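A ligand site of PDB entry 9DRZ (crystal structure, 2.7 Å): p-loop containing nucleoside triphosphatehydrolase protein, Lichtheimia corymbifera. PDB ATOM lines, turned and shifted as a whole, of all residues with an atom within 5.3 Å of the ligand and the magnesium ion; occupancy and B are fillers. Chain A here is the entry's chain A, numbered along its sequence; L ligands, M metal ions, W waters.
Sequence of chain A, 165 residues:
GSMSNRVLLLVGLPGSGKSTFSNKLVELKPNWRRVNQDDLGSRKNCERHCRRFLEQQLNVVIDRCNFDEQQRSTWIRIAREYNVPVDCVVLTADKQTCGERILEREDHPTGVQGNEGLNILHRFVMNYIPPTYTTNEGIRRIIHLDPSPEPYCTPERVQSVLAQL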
ATOM      1  N   LEU A  13      22.592   7.924 -20.825  1.00  0.00           N
ATOM      2  CA  LEU A  13      22.628   7.266 -19.527  1.00  0.00           C
ATOM      3  C   LEU A  13      22.295   8.291 -18.464  1.00  0.00           C
ATOM      4  O   LEU A  13      22.482   9.492 -18.645  1.00  0.00           O
ATOM      5  CB  LEU A  13      24.019   6.694 -19.301  1.00  0.00           C
ATOM      6  CG  LEU A  13      24.440   5.578 -20.249  1.00  0.00           C
ATOM      7  CD1 LEU A  13      25.935   5.285 -20.094  1.00  0.00           C
ATOM      8  CD2 LEU A  13      23.588   4.327 -20.023  1.00  0.00           C
ATOM      9  N   PRO A  14      21.820   7.844 -17.283  1.00  0.00           N
ATOM     10  CA  PRO A  14      21.759   8.709 -16.105  1.00  0.00           C
ATOM     11  C   PRO A  14      23.082   9.450 -15.951  1.00  0.00           C
ATOM     12  O   PRO A  14      24.157   8.845 -16.068  1.00  0.00           O
ATOM     13  CB  PRO A  14      21.501   7.728 -14.982  1.00  0.00           C
ATOM     14  CG  PRO A  14      20.747   6.599 -15.639  1.00  0.00           C
ATOM     15  CD  PRO A  14      21.339   6.486 -17.035  1.00  0.00           C
ATOM     16  N   GLY A  15      23.001  10.762 -15.744  1.00  0.00           N
ATOM     17  CA  GLY A  15      24.158  11.607 -15.495  1.00  0.00           C
ATOM     18  C   GLY A  15      24.912  11.976 -16.765  1.00  0.00           C
ATOM     19  O   GLY A  15      26.032  12.469 -16.687  1.00  0.00           O
ATOM     20  N   SER A  16      24.313  11.768 -17.942  1.00  0.00           N
ATOM     21  CA  SER A  16      25.008  12.074 -19.184  1.00  0.00           C
ATOM     22  C   SER A  16      24.945  13.581 -19.467  1.00  0.00           C
ATOM     23  O   SER A  16      25.872  14.118 -20.069  1.00  0.00           O
ATOM     24  CB  SER A  16      24.482  11.252 -20.338  1.00  0.00           C
ATOM     25  OG  SER A  16      23.073  11.158 -20.326  1.00  0.00           O
ATOM     26  N   GLY A  17      23.883  14.254 -19.030  1.00  0.00           N
ATOM     27  CA  GLY A  17      23.783  15.707 -19.152  1.00  0.00           C
ATOM     28  C   GLY A  17      22.550  16.169 -19.926  1.00  0.00           C
ATOM     29  O   GLY A  17      22.558  17.254 -20.523  1.00  0.00           O
ATOM     30  N   LYS A  18      21.485  15.364 -19.875  1.00  0.00           N
ATOM     31  CA  LYS A  18      20.290  15.577 -20.692  1.00  0.00           C
ATOM     32  C   LYS A  18      19.529  16.804 -20.182  1.00  0.00           C
ATOM     33  O   LYS A  18      19.080  17.637 -20.955  1.00  0.00           O
ATOM     34  CB  LYS A  18      19.393  14.345 -20.603  1.00  0.00           C
ATOM     35  CG  LYS A  18      20.016  13.013 -21.012  1.00  0.00           C
ATOM     36  CD  LYS A  18      19.098  11.804 -20.864  1.00  0.00           C
ATOM     37  CE  LYS A  18      18.659  11.475 -19.443  1.00  0.00           C
ATOM     38  NZ  LYS A  18      19.655  10.826 -18.579  1.00  0.00           N
ATOM     39  N   SER A  19      19.383  16.893 -18.863  1.00  0.00           N
ATOM     40  CA  SER A  19      18.727  18.035 -18.248  1.00  0.00           C
ATOM     41  C   SER A  19      19.582  19.291 -18.445  1.00  0.00           C
ATOM     42  O   SER A  19      19.063  20.345 -18.816  1.00  0.00           O
ATOM     43  CB  SER A  19      18.452  17.761 -16.798  1.00  0.00           C
ATOM     44  OG  SER A  19      17.817  16.493 -16.658  1.00  0.00           O
ATOM     45  N   THR A  20      20.895  19.170 -18.207  1.00  0.00           N
ATOM     46  CA  THR A  20      21.808  20.272 -18.467  1.00  0.00           C
ATOM     47  C   THR A  20      21.431  20.894 -19.807  1.00  0.00           C
ATOM     48  O   THR A  20      21.152  22.078 -19.882  1.00  0.00           O
ATOM     49  CB  THR A  20      23.262  19.803 -18.459  1.00  0.00           C
ATOM     50  OG1 THR A  20      23.553  19.408 -17.112  1.00  0.00           O
ATOM     51  CG2 THR A  20      24.241  20.888 -18.864  1.00  0.00           C
ATOM     52  N   PHE A  21      21.373  20.063 -20.859  1.00  0.00           N
ATOM     53  CA  PHE A  21      21.171  20.549 -22.209  1.00  0.00           C
ATOM     54  C   PHE A  21      19.749  21.072 -22.432  1.00  0.00           C
ATOM     55  O   PHE A  21      19.581  22.153 -22.987  1.00  0.00           O
ATOM     56  CB  PHE A  21      21.442  19.433 -23.218  1.00  0.00           C
ATOM     57  CG  PHE A  21      21.269  19.920 -24.644  1.00  0.00           C
ATOM     58  CD1 PHE A  21      22.311  20.567 -25.298  1.00  0.00           C
ATOM     59  CD2 PHE A  21      20.075  19.727 -25.328  1.00  0.00           C
ATOM     60  CE1 PHE A  21      22.167  21.003 -26.611  1.00  0.00           C
ATOM     61  CE2 PHE A  21      19.931  20.163 -26.641  1.00  0.00           C
ATOM     62  CZ  PHE A  21      20.975  20.797 -27.277  1.00  0.00           C
ATOM     63  N   ASN A  36       9.914  16.616 -18.753  1.00  0.00           N
ATOM     64  CA  ASN A  36      10.789  15.908 -17.840  1.00  0.00           C
ATOM     65  C   ASN A  36       9.908  15.272 -16.773  1.00  0.00           C
ATOM     66  O   ASN A  36       8.975  15.918 -16.307  1.00  0.00           O
ATOM     67  CB  ASN A  36      11.816  16.822 -17.207  1.00  0.00           C
ATOM     68  CG  ASN A  36      12.591  16.129 -16.124  1.00  0.00           C
ATOM     69  OD1 ASN A  36      12.602  16.569 -14.978  1.00  0.00           O
ATOM     70  ND2 ASN A  36      13.265  15.043 -16.458  1.00  0.00           N
ATOM     71  N   ASP A  38      10.652  14.224 -13.767  1.00  0.00           N
ATOM     72  CA  ASP A  38      10.969  14.651 -12.387  1.00  0.00           C
ATOM     73  C   ASP A  38      10.170  15.907 -12.085  1.00  0.00           C
ATOM     74  O   ASP A  38      10.013  16.254 -10.907  1.00  0.00           O
ATOM     75  CB  ASP A  38      12.463  14.836 -12.215  1.00  0.00           C
ATOM     76  CG  ASP A  38      13.285  13.557 -12.336  1.00  0.00           C
ATOM     77  OD1 ASP A  38      12.820  12.517 -11.825  1.00  0.00           O
ATOM     78  OD2 ASP A  38      14.377  13.625 -12.927  1.00  0.00           O
ATOM     79  N   ASP A  63      13.207  15.147 -22.111  1.00  0.00           N
ATOM     80  CA  ASP A  63      14.369  14.909 -21.216  1.00  0.00           C
ATOM     81  C   ASP A  63      14.157  13.587 -20.474  1.00  0.00           C
ATOM     82  O   ASP A  63      13.806  13.625 -19.280  1.00  0.00           O
ATOM     83  CB  ASP A  63      14.577  16.115 -20.315  1.00  0.00           C
ATOM     84  CG  ASP A  63      15.636  15.977 -19.233  1.00  0.00           C
ATOM     85  OD1 ASP A  63      16.661  15.322 -19.489  1.00  0.00           O
ATOM     86  OD2 ASP A  63      15.426  16.530 -18.130  1.00  0.00           O
ATOM     87  N   ARG A 101      30.190  11.635 -12.395  1.00  0.00           N
ATOM     88  CA  ARG A 101      29.182  12.665 -12.165  1.00  0.00           C
ATOM     89  C   ARG A 101      28.203  12.237 -11.081  1.00  0.00           C
ATOM     90  O   ARG A 101      27.793  13.060 -10.269  1.00  0.00           O
ATOM     91  CB  ARG A 101      28.416  12.980 -13.456  1.00  0.00           C
ATOM     92  CG  ARG A 101      29.315  13.583 -14.531  1.00  0.00           C
ATOM     93  CD  ARG A 101      28.584  13.705 -15.839  1.00  0.00           C
ATOM     94  NE  ARG A 101      29.359  14.381 -16.885  1.00  0.00           N
ATOM     95  CZ  ARG A 101      28.939  14.507 -18.136  1.00  0.00           C
ATOM     96  NH1 ARG A 101      27.720  14.115 -18.454  1.00  0.00           N
ATOM     97  NH2 ARG A 101      29.727  15.045 -19.060  1.00  0.00           N
ATOM     98  N   ASP A 146      28.906  15.036 -27.875  1.00  0.00           N
ATOM     99  CA  ASP A 146      29.986  14.727 -26.955  1.00  0.00           C
ATOM    100  C   ASP A 146      29.914  15.674 -25.755  1.00  0.00           C
ATOM    101  O   ASP A 146      29.411  16.788 -25.869  1.00  0.00           O
ATOM    102  CB  ASP A 146      31.324  14.810 -27.647  1.00  0.00           C
ATOM    103  CG  ASP A 146      31.543  13.770 -28.734  1.00  0.00           C
ATOM    104  OD1 ASP A 146      31.391  12.568 -28.424  1.00  0.00           O
ATOM    105  OD2 ASP A 146      31.860  14.189 -29.875  1.00  0.00           O
ATOM    106  N   PRO A 147      30.414  15.265 -24.573  1.00  0.00           N
ATOM    107  CA  PRO A 147      30.498  16.178 -23.427  1.00  0.00           C
ATOM    108  C   PRO A 147      31.374  17.403 -23.689  1.00  0.00           C
ATOM    109  O   PRO A 147      32.397  17.331 -24.353  1.00  0.00           O
ATOM    110  CB  PRO A 147      31.066  15.287 -22.313  1.00  0.00           C
ATOM    111  CG  PRO A 147      30.742  13.876 -22.757  1.00  0.00           C
ATOM    112  CD  PRO A 147      30.900  13.912 -24.270  1.00  0.00           C
ATOM    113  N   SER A 148      30.943  18.548 -23.154  1.00  0.00           N
ATOM    114  CA  SER A 148      31.745  19.770 -23.164  1.00  0.00           C
ATOM    115  C   SER A 148      32.776  19.735 -22.034  1.00  0.00           C
ATOM    116  O   SER A 148      32.590  19.035 -21.041  1.00  0.00           O
ATOM    117  CB  SER A 148      30.858  20.985 -23.067  1.00  0.00           C
ATOM    118  OG  SER A 148      29.940  20.875 -21.981  1.00  0.00           O
ATOM    119  N   PRO A 149      33.908  20.488 -22.141  1.00  0.00           N
ATOM    120  CA  PRO A 149      34.804  20.692 -21.002  1.00  0.00           C
ATOM    121  C   PRO A 149      34.057  21.326 -19.830  1.00  0.00           C
ATOM    122  O   PRO A 149      34.310  20.960 -18.692  1.00  0.00           O
ATOM    123  CB  PRO A 149      35.913  21.614 -21.517  1.00  0.00           C
ATOM    124  CG  PRO A 149      35.801  21.569 -23.028  1.00  0.00           C
ATOM    125  CD  PRO A 149      34.365  21.182 -23.353  1.00  0.00           C
ATOM    126  N   GLU A 150      33.132  22.235 -20.142  1.00  0.00           N
ATOM    127  CA  GLU A 150      32.435  23.033 -19.137  1.00  0.00           C
ATOM    128  C   GLU A 150      31.260  22.253 -18.560  1.00  0.00           C
ATOM    129  O   GLU A 150      30.503  21.648 -19.310  1.00  0.00           O
ATOM    130  CB  GLU A 150      31.859  24.335 -19.721  1.00  0.00           C
ATOM    131  CG  GLU A 150      32.841  25.147 -20.572  1.00  0.00           C
ATOM    132  CD  GLU A 150      32.892  24.779 -22.041  1.00  0.00           C
ATOM    133  OE1 GLU A 150      32.925  23.569 -22.327  1.00  0.00           O
ATOM    134  OE2 GLU A 150      32.927  25.680 -22.926  1.00  0.00           O
ATOM    135  N   PRO A 151      31.049  22.275 -17.224  1.00  0.00           N
ATOM    136  CA  PRO A 151      29.839  21.698 -16.626  1.00  0.00           C
ATOM    137  C   PRO A 151      28.539  22.323 -17.111  1.00  0.00           C
ATOM    138  O   PRO A 151      27.520  21.663 -17.179  1.00  0.00           O
ATOM    139  CB  PRO A 151      30.043  21.943 -15.118  1.00  0.00           C
ATOM    140  CG  PRO A 151      31.549  22.045 -14.968  1.00  0.00           C
ATOM    141  CD  PRO A 151      31.972  22.807 -16.208  1.00  0.00           C
ATOM    142  N   TYR A 152      28.591  23.609 -17.431  1.00  0.00           N
ATOM    143  CA  TYR A 152      27.410  24.317 -17.890  1.00  0.00           C
ATOM    144  C   TYR A 152      27.355  24.253 -19.414  1.00  0.00           C
ATOM    145  O   TYR A 152      28.365  24.100 -20.081  1.00  0.00           O
ATOM    146  CB  TYR A 152      27.440  25.764 -17.404  1.00  0.00           C
ATOM    147  CG  TYR A 152      28.704  26.513 -17.811  1.00  0.00           C
ATOM    148  CD1 TYR A 152      29.844  26.476 -17.003  1.00  0.00           C
ATOM    149  CD2 TYR A 152      28.768  27.228 -19.001  1.00  0.00           C
ATOM    150  CE1 TYR A 152      30.999  27.146 -17.370  1.00  0.00           C
ATOM    151  CE2 TYR A 152      29.923  27.889 -19.374  1.00  0.00           C
ATOM    152  CZ  TYR A 152      31.038  27.853 -18.547  1.00  0.00           C
ATOM    153  OH  TYR A 152      32.171  28.522 -18.912  1.00  0.00           O
ATOM    154  N   ARG A 157      26.818  26.002 -27.803  1.00  0.00           N
ATOM    155  CA  ARG A 157      26.651  24.553 -27.849  1.00  0.00           C
ATOM    156  C   ARG A 157      25.226  24.201 -28.285  1.00  0.00           C
ATOM    157  O   ARG A 157      25.033  23.319 -29.117  1.00  0.00           O
ATOM    158  CB  ARG A 157      26.988  24.006 -26.455  1.00  0.00           C
ATOM    159  CG  ARG A 157      26.846  22.502 -26.288  1.00  0.00           C
ATOM    160  CD  ARG A 157      27.325  22.142 -24.901  1.00  0.00           C
ATOM    161  NE  ARG A 157      27.080  20.752 -24.495  1.00  0.00           N
ATOM    162  CZ  ARG A 157      27.768  19.706 -24.911  1.00  0.00           C
ATOM    163  NH1 ARG A 157      28.652  19.810 -25.891  1.00  0.00           N
ATOM    164  NH2 ARG A 157      27.561  18.531 -24.342  1.00  0.00           N
HETATM  165  P1  LIG L   1      20.987  13.834 -16.693  1.00  0.00           P
HETATM  166  O1  LIG L   1      20.847  12.933 -15.503  1.00  0.00           O
HETATM  167  O2  LIG L   1      19.792  14.702 -16.918  1.00  0.00           O
HETATM  168  O3  LIG L   1      21.437  13.149 -17.964  1.00  0.00           O
HETATM  169  O4  LIG L   1      22.290  14.691 -16.273  1.00  0.00           O
HETATM  170  P2  LIG L   1      22.426  16.184 -15.719  1.00  0.00           P
HETATM  171  O5  LIG L   1      21.879  17.100 -16.761  1.00  0.00           O
HETATM  172  O6  LIG L   1      21.850  16.156 -14.347  1.00  0.00           O
HETATM  173  O7  LIG L   1      24.007  16.376 -15.622  1.00  0.00           O
HETATM  174  C1  LIG L   1      24.749  15.589 -14.650  1.00  0.00           C
HETATM  175  C2  LIG L   1      26.035  16.282 -14.288  1.00  0.00           C
HETATM  176  O8  LIG L   1      26.929  16.315 -15.437  1.00  0.00           O
HETATM  177  C3  LIG L   1      25.900  17.740 -13.841  1.00  0.00           C
HETATM  178  O9  LIG L   1      26.825  18.039 -12.815  1.00  0.00           O
HETATM  179  C4  LIG L   1      26.306  18.551 -15.063  1.00  0.00           C
HETATM  180  O10 LIG L   1      26.913  19.744 -14.623  1.00  0.00           O
HETATM  181  C5  LIG L   1      27.307  17.635 -15.764  1.00  0.00           C
HETATM  182  N1  LIG L   1      27.304  17.771 -17.216  1.00  0.00           N
HETATM  183  C6  LIG L   1      26.208  17.701 -18.045  1.00  0.00           C
HETATM  184  N2  LIG L   1      26.500  17.874 -19.321  1.00  0.00           N
HETATM  185  C7  LIG L   1      27.873  18.061 -19.328  1.00  0.00           C
HETATM  186  C8  LIG L   1      28.760  18.289 -20.409  1.00  0.00           C
HETATM  187  O11 LIG L   1      28.497  18.393 -21.621  1.00  0.00           O
HETATM  188  N3  LIG L   1      30.069  18.433 -19.972  1.00  0.00           N
HETATM  189  C9  LIG L   1      30.481  18.372 -18.657  1.00  0.00           C
HETATM  190  N4  LIG L   1      31.791  18.550 -18.439  1.00  0.00           N
HETATM  191  N5  LIG L   1      29.657  18.152 -17.630  1.00  0.00           N
HETATM  192  C10 LIG L   1      28.373  18.013 -18.040  1.00  0.00           C
HETATM  193 MG    MG M   1      18.215  14.779 -15.713  1.00  0.00          MG
HETATM  194  O   HOH W   1      18.483  13.143 -14.619  1.00  0.00           O
HETATM  195  O   HOH W   2      16.577  14.940 -14.576  1.00  0.00           O
HETATM  196  O   HOH W   3      19.145  15.866 -14.321  1.00  0.00           O
HETATM  197  O   HOH W   4      16.855  13.999 -16.932  1.00  0.00           O
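O of Pro 149 is in hydrogen-bond range of N4 of the ligand, 3.5 Å away.
A nitrogen (N4) of the ligand is in hydrogen-bond range of the backbone carbonyl oxygen (O) of Ser 148 (2.8 Å).
The side-chain hydroxyl (OG1) of Thr 20 sits at hydrogen-bond distance from an oxygen (O5) of the ligand.
The backbone NH of Ser 19 lies within hydrogen-bond range of an oxygen (O5) of the ligand (3.3 Å).
The backbone carbonyl oxygen (O) of Pro 151 sits at hydrogen-bond distance from an oxygen (O10) of the ligand (3.3 Å).
N of Lys 18 sits at hydrogen-bond distance from O3 of the ligand (2.9 Å).
N5 of the ligand lies close to NH2 of Arg 101 (3.4 Å).
OG of Ser 148 lies within hydrogen-bond range of O11 of the ligand, 2.9 Å away.
An oxygen (O11) of the ligand lies within hydrogen-bond range of the backbone NH (N) of Ser 148, 2.9 Å away.
The backbone NH of Gly 15 is in hydrogen-bond range of an oxygen (O1) of the ligand (3.1 Å).
The guanidinium group of Arg 157 is in hydrogen-bond range of an oxygen (O11) of the ligand, 2.9 Å away.
N of Gly 17 sits at hydrogen-bond distance from O3 of the ligand (2.9 Å).
An oxygen (O3) of the ligand sits at hydrogen-bond distance from the backbone NH (N) of Ser 16, at 3.2 Å.
An oxygen (O5) of the ligand is in hydrogen-bond range of the backbone NH (N) of Thr 20 (2.7 Å).
The side-chain hydroxyl of Ser 16 lies within hydrogen-bond range of an oxygen (O3) of the ligand, at 3.5 Å.
The side-chain amino group of Lys 18 lies within salt-bridge range of an oxygen (O3) of the ligand (3.0 Å).
N3 of the ligand lies within hydrogen-bond range of O of Glu 150 (3.3 Å).
O of Leu 13 touches O3 of the ligand (3.9 Å).
Pro 147 touches the ligand.
Hydrophobic or aromatic side chains within 4 Å of the ligand: Pro 151.
14 residues have an atom within 4 Å of the ligand: Leu 13, Gly 15, Ser 16, Gly 17, Lys 18, Ser 19, Thr 20, Arg 101, Pro 147, Ser 148, Pro 149, Glu 150, Pro 151 and Arg 157.
The nearest printed residue that does not touch the ligand is Asp 63 (4.1 Å).
O of Glu 150 is in hydrogen-bond range of OG of Ser 148 (2.8 Å).
The backbone carbonyl oxygen (O) of Leu 13 sits at hydrogen-bond distance from the side-chain amino group (NZ) of Lys 18 (3.1 Å).
The side-chain hydroxyl (OG) of Ser 16 sits at hydrogen-bond distance from the backbone carbonyl oxygen (O) of Leu 13.
O of Gly 15 lies within hydrogen-bond range of NH1 of Arg 101.
The guanidinium group of Arg 157 lies within hydrogen-bond range of the backbone carbonyl oxygen of Asp 146 (3.0 Å).
The backbone NH (N) of Ser 19 sits at hydrogen-bond distance from the side-chain carboxylate (OD1) of Asp 63 (3.2 Å).
The backbone carbonyl oxygen (O) of Ser 16 lies within hydrogen-bond range of the guanidinium group (NH1) of Arg 101.
The magnesium ion is bound by O2 of the ligand.
Water W4 is bound to the magnesium ion, at 2.0 Å.
Water W1 is bound to the magnesium ion (2.0 Å).
Water W3 is bound to the magnesium ion, at 2.0 Å.
The magnesium ion is bound by OG of Ser 19 (2.0 Å).
Water W2 is bound to the magnesium ion.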
